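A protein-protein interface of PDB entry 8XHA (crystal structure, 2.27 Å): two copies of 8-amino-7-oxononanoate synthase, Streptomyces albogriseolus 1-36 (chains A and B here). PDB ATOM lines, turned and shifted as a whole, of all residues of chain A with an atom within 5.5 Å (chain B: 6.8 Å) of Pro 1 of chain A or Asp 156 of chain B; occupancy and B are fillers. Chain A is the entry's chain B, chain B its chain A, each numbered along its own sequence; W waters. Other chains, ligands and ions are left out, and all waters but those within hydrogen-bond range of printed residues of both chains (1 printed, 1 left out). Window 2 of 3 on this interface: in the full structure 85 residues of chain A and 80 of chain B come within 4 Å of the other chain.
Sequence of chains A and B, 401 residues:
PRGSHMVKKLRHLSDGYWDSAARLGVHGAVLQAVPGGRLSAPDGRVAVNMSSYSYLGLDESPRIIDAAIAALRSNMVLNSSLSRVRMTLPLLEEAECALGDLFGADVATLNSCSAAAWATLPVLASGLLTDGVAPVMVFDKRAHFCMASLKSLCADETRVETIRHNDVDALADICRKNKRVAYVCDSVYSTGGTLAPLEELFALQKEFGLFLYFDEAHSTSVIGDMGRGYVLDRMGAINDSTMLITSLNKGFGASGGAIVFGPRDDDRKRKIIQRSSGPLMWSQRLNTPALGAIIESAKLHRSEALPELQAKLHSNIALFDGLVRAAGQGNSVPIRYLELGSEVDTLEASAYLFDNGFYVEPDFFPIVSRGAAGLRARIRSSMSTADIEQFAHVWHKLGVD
The side-chain hydroxyl (OG) of Ser 152 of chain B lies close to the side-chain carboxylate (OD1) of Asp 156 of chain A, 3.1 Å away. OD2 of Asp 156 of chain B lies within hydrogen-bond range of OG of Ser 152 of chain A (2.4 Å). The side-chain sulfur (SD) of Met 6 of chain A lies close to the backbone carbonyl oxygen (O) of Asp 156 of chain B (3.7 Å).
Ser 152 of chain B touches its own counterpart, Ser 152 of chain A. Ser 152 of chain A touches Asp 156 of chain B, and with the chains exchanged Asp 156 of chain A touches Ser 152 of chain B. Of the 8 pairs that touch across the chains among the printed residues, 3 have their exchanged pair printed and touching as well.
Pro 1 of chain A touches Asp 156 of chain B (O to OD1, 3.8 Å). Asp 156 of chain B touches Ser 4 of chain A. Met 6 of chain A touches Glu 157 of chain B. Ser 152 of chain B touches Ser 152 of chain A. Ser 152 of chain A touches Leu 153 of chain B (CB to CD2, 3.9 Å).
Pro 1 of chain A touches one residue of chain B. Gly 3 of chain A touches none of the printed residues of chain B. Of the printed residues of chain B, Ser 152 of chain A touches Ser 152 (3.98 Å), Leu 153 (3.9 Å) and Asp 156 (2.4 Å). Printed residues of chain B within 4 Å of Asp 156 of chain A: Ser 152. Printed residues of chain A within 4 Å of Ser 152 of chain B: Ser 152 (3.98 Å) and Asp 156 (2.3 Å). Of the printed residues of chain A, Leu 153 of chain B touches Ser 152. The nearest residue of chain A that does not touch Asp 156 of chain B is Gly 3 of chain A (4.1 Å).
Of the 10 printed residues of chain B, 4 touch a printed residue of chain A. Printed residues of chain B that touch a printed residue of chain A: Ser 152, Leu 153, Asp 156 and Glu 157. Of the 9 printed residues of chain A, 5 touch a printed residue of chain B. Hydrophobic or aromatic side chains of chain A that line the printed part of chain B: Met 6. Among the printed residues, 8 pairs touch across the chains. Among the printed residues, no Asp or Glu carboxylate lies within 4 Å of a Lys or Arg side-chain nitrogen of the other chain.
OG of Ser 152 of chain A is in hydrogen-bond range of O of Gly 3 of chain A.
Water W1 lies within hydrogen-bond range of the backbone NH of His 5 of chain A (3.1 Å), the side-chain carboxylate of Asp 156 of chain B (3.3 Å) and the side-chain hydroxyl of Ser 152 of chain A (3.3 Å).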
ATOM      1  N   PRO A   1      19.232   6.262 -12.934  1.00  0.00           N
ATOM      2  CA  PRO A   1      20.092   7.319 -13.492  1.00  0.00           C
ATOM      3  C   PRO A   1      20.290   8.539 -12.571  1.00  0.00           C
ATOM      4  O   PRO A   1      20.730   8.328 -11.461  1.00  0.00           O
ATOM      5  CB  PRO A   1      19.355   7.700 -14.780  1.00  0.00           C
ATOM      6  CG  PRO A   1      18.818   6.382 -15.271  1.00  0.00           C
ATOM      7  CD  PRO A   1      18.466   5.623 -14.008  1.00  0.00           C
ATOM      8  N   ARG A   2      19.972   9.761 -13.009  1.00  0.00           N
ATOM      9  CA  ARG A   2      20.295  10.968 -12.181  1.00  0.00           C
ATOM     10  C   ARG A   2      19.654  10.910 -10.787  1.00  0.00           C
ATOM     11  O   ARG A   2      20.417  10.898  -9.806  1.00  0.00           O
ATOM     12  CB  ARG A   2      19.906  12.278 -12.869  1.00  0.00           C
ATOM     13  CG  ARG A   2      20.426  13.502 -12.129  1.00  0.00           C
ATOM     14  CD  ARG A   2      20.176  14.828 -12.817  1.00  0.00           C
ATOM     15  NE  ARG A   2      20.794  15.909 -12.064  1.00  0.00           N
ATOM     16  CZ  ARG A   2      20.628  17.199 -12.327  1.00  0.00           C
ATOM     17  NH1 ARG A   2      19.852  17.575 -13.329  1.00  0.00           N
ATOM     18  NH2 ARG A   2      21.231  18.106 -11.580  1.00  0.00           N
ATOM     19  N   GLY A   3      18.322  10.916 -10.695  1.00  0.00           N
ATOM     20  CA  GLY A   3      17.676  10.773  -9.377  1.00  0.00           C
ATOM     21  C   GLY A   3      18.214   9.554  -8.661  1.00  0.00           C
ATOM     22  O   GLY A   3      18.377   8.523  -9.329  1.00  0.00           O
ATOM     23  N   SER A   4      18.494   9.660  -7.358  1.00  0.00           N
ATOM     24  CA  SER A   4      19.142   8.512  -6.673  1.00  0.00           C
ATOM     25  C   SER A   4      18.926   8.515  -5.159  1.00  0.00           C
ATOM     26  O   SER A   4      18.526   9.559  -4.623  1.00  0.00           O
ATOM     27  CB  SER A   4      20.609   8.484  -6.992  1.00  0.00           C
ATOM     28  OG  SER A   4      21.266   9.611  -6.434  1.00  0.00           O
ATOM     29  N   HIS A   5      19.168   7.374  -4.514  1.00  0.00           N
ATOM     30  CA  HIS A   5      19.090   7.242  -3.037  1.00  0.00           C
ATOM     31  C   HIS A   5      20.313   6.408  -2.673  1.00  0.00           C
ATOM     32  O   HIS A   5      20.133   5.223  -2.341  1.00  0.00           O
ATOM     33  CB  HIS A   5      17.762   6.603  -2.633  1.00  0.00           C
ATOM     34  CG  HIS A   5      17.418   6.699  -1.186  1.00  0.00           C
ATOM     35  ND1 HIS A   5      16.842   7.827  -0.640  1.00  0.00           N
ATOM     36  CD2 HIS A   5      17.521   5.802  -0.183  1.00  0.00           C
ATOM     37  CE1 HIS A   5      16.626   7.628   0.643  1.00  0.00           C
ATOM     38  NE2 HIS A   5      17.033   6.394   0.947  1.00  0.00           N
ATOM     39  N   MET A   6      21.505   6.999  -2.750  1.00  0.00           N
ATOM     40  CA  MET A   6      22.769   6.233  -2.580  1.00  0.00           C
ATOM     41  C   MET A   6      22.959   5.678  -1.170  1.00  0.00           C
ATOM     42  O   MET A   6      22.550   6.338  -0.212  1.00  0.00           O
ATOM     43  CB  MET A   6      23.961   7.132  -2.916  1.00  0.00           C
ATOM     44  CG  MET A   6      23.839   7.843  -4.248  1.00  0.00           C
ATOM     45  SD  MET A   6      24.211   6.778  -5.657  1.00  0.00           S
ATOM     46  CE  MET A   6      25.795   6.110  -5.156  1.00  0.00           C
ATOM     47  N   SER A 152      15.727   5.911  -8.746  1.00  0.00           N
ATOM     48  CA  SER A 152      16.543   5.356  -9.856  1.00  0.00           C
ATOM     49  C   SER A 152      15.672   4.519 -10.797  1.00  0.00           C
ATOM     50  O   SER A 152      15.899   4.580 -12.009  1.00  0.00           O
ATOM     51  CB  SER A 152      17.693   4.559  -9.328  1.00  0.00           C
ATOM     52  OG  SER A 152      18.455   5.325  -8.413  1.00  0.00           O
ATOM     53  N   ALA A 155      13.755   6.896 -12.797  1.00  0.00           N
ATOM     54  CA  ALA A 155      14.637   7.602 -13.754  1.00  0.00           C
ATOM     55  C   ALA A 155      14.918   6.705 -14.955  1.00  0.00           C
ATOM     56  O   ALA A 155      15.246   7.236 -16.019  1.00  0.00           O
ATOM     57  CB  ALA A 155      15.913   8.005 -13.070  1.00  0.00           C
ATOM     58  N   ASP A 156      14.808   5.395 -14.769  1.00  0.00           N
ATOM     59  CA  ASP A 156      14.975   4.453 -15.896  1.00  0.00           C
ATOM     60  C   ASP A 156      13.820   4.652 -16.880  1.00  0.00           C
ATOM     61  O   ASP A 156      13.930   4.174 -18.016  1.00  0.00           O
ATOM     62  CB  ASP A 156      15.020   3.015 -15.390  1.00  0.00           C
ATOM     63  CG  ASP A 156      16.416   2.460 -15.204  1.00  0.00           C
ATOM     64  OD1 ASP A 156      17.368   3.252 -15.228  1.00  0.00           O
ATOM     65  OD2 ASP A 156      16.533   1.234 -15.051  1.00  0.00           O
ATOM     66  N   ALA B 125      25.856  -4.130  -3.429  1.00  0.00           N
ATOM     67  CA  ALA B 125      26.414  -3.366  -4.541  1.00  0.00           C
ATOM     68  C   ALA B 125      27.352  -2.255  -4.072  1.00  0.00           C
ATOM     69  O   ALA B 125      28.291  -1.893  -4.797  1.00  0.00           O
ATOM     70  CB  ALA B 125      25.288  -2.768  -5.376  1.00  0.00           C
ATOM     71  N   LYS B 151      18.014  -3.636 -10.419  1.00  0.00           N
ATOM     72  CA  LYS B 151      19.335  -3.446 -11.016  1.00  0.00           C
ATOM     73  C   LYS B 151      19.723  -1.976 -11.046  1.00  0.00           C
ATOM     74  O   LYS B 151      20.895  -1.632 -10.866  1.00  0.00           O
ATOM     75  CB  LYS B 151      19.375  -4.022 -12.431  1.00  0.00           C
ATOM     76  CG  LYS B 151      19.476  -5.530 -12.513  1.00  0.00           C
ATOM     77  CD  LYS B 151      19.265  -5.980 -13.970  1.00  0.00           C
ATOM     78  CE  LYS B 151      19.375  -7.490 -14.109  1.00  0.00           C
ATOM     79  NZ  LYS B 151      18.936  -7.978 -15.445  1.00  0.00           N
ATOM     80  N   SER B 152      18.761  -1.091 -11.279  1.00  0.00           N
ATOM     81  CA  SER B 152      19.097   0.325 -11.301  1.00  0.00           C
ATOM     82  C   SER B 152      19.643   0.791  -9.960  1.00  0.00           C
ATOM     83  O   SER B 152      20.610   1.563  -9.920  1.00  0.00           O
ATOM     84  CB  SER B 152      17.890   1.150 -11.709  1.00  0.00           C
ATOM     85  OG  SER B 152      17.692   0.983 -13.093  1.00  0.00           O
ATOM     86  N   LEU B 153      19.049   0.336  -8.851  1.00  0.00           N
ATOM     87  CA  LEU B 153      19.597   0.704  -7.549  1.00  0.00           C
ATOM     88  C   LEU B 153      21.044   0.253  -7.438  1.00  0.00           C
ATOM     89  O   LEU B 153      21.899   0.991  -6.937  1.00  0.00           O
ATOM     90  CB  LEU B 153      18.776   0.102  -6.405  1.00  0.00           C
ATOM     91  CG  LEU B 153      17.285   0.398  -6.264  1.00  0.00           C
ATOM     92  CD1 LEU B 153      16.791   0.089  -4.827  1.00  0.00           C
ATOM     93  CD2 LEU B 153      16.986   1.818  -6.632  1.00  0.00           C
ATOM     94  N   CYS B 154      21.339  -0.954  -7.915  1.00  0.00           N
ATOM     95  CA  CYS B 154      22.702  -1.457  -7.865  1.00  0.00           C
ATOM     96  C   CYS B 154      23.620  -0.692  -8.823  1.00  0.00           C
ATOM     97  O   CYS B 154      24.785  -0.432  -8.497  1.00  0.00           O
ATOM     98  CB  CYS B 154      22.703  -2.940  -8.190  1.00  0.00           C
ATOM     99  SG  CYS B 154      21.675  -3.900  -7.067  1.00  0.00           S
ATOM    100  N   ALA B 155      23.112  -0.331 -10.006  1.00  0.00           N
ATOM    101  CA  ALA B 155      23.953   0.337 -10.991  1.00  0.00           C
ATOM    102  C   ALA B 155      24.436   1.683 -10.480  1.00  0.00           C
ATOM    103  O   ALA B 155      25.556   2.093 -10.801  1.00  0.00           O
ATOM    104  CB  ALA B 155      23.212   0.511 -12.315  1.00  0.00           C
ATOM    105  N   ASP B 156      23.622   2.366  -9.661  1.00  0.00           N
ATOM    106  CA  ASP B 156      24.070   3.603  -9.030  1.00  0.00           C
ATOM    107  C   ASP B 156      25.269   3.388  -8.122  1.00  0.00           C
ATOM    108  O   ASP B 156      26.004   4.343  -7.849  1.00  0.00           O
ATOM    109  CB  ASP B 156      22.940   4.236  -8.224  1.00  0.00           C
ATOM    110  CG  ASP B 156      21.893   4.868  -9.101  1.00  0.00           C
ATOM    111  OD1 ASP B 156      22.107   4.915 -10.334  1.00  0.00           O
ATOM    112  OD2 ASP B 156      20.859   5.307  -8.562  1.00  0.00           O
ATOM    113  N   GLU B 157      25.481   2.168  -7.646  1.00  0.00           N
ATOM    114  CA  GLU B 157      26.581   1.882  -6.745  1.00  0.00           C
ATOM    115  C   GLU B 157      27.821   1.349  -7.453  1.00  0.00           C
ATOM    116  O   GLU B 157      28.938   1.603  -6.988  1.00  0.00           O
ATOM    117  CB  GLU B 157      26.135   0.864  -5.690  1.00  0.00           C
ATOM    118  CG  GLU B 157      24.919   1.309  -4.864  1.00  0.00           C
ATOM    119  CD  GLU B 157      25.239   2.451  -3.910  1.00  0.00           C
ATOM    120  OE1 GLU B 157      26.432   2.652  -3.607  1.00  0.00           O
ATOM    121  OE2 GLU B 157      24.304   3.155  -3.465  1.00  0.00           O
ATOM    122  N   THR B 158      27.659   0.642  -8.567  1.00  0.00           N
ATOM    123  CA  THR B 158      28.739  -0.156  -9.121  1.00  0.00           C
ATOM    124  C   THR B 158      28.354  -0.627 -10.522  1.00  0.00           C
ATOM    125  O   THR B 158      27.336  -0.176 -11.090  1.00  0.00           O
ATOM    126  CB  THR B 158      29.052  -1.329  -8.177  1.00  0.00           C
ATOM    127  OG1 THR B 158      30.136  -2.100  -8.709  1.00  0.00           O
ATOM    128  CG2 THR B 158      27.810  -2.225  -8.040  1.00  0.00           C
ATOM    129  N   VAL B 160      26.868  -3.222 -13.125  1.00  0.00           N
ATOM    130  CA  VAL B 160      25.886  -4.297 -13.163  1.00  0.00           C
ATOM    131  C   VAL B 160      26.008  -5.011 -14.498  1.00  0.00           C
ATOM    132  O   VAL B 160      25.976  -4.372 -15.555  1.00  0.00           O
ATOM    133  CB  VAL B 160      24.460  -3.764 -12.954  1.00  0.00           C
ATOM    134  CG1 VAL B 160      23.449  -4.875 -13.181  1.00  0.00           C
ATOM    135  CG2 VAL B 160      24.315  -3.193 -11.561  1.00  0.00           C
HETATM  136  O   HOH W   1      19.940   4.548  -5.538  1.00  0.00           O
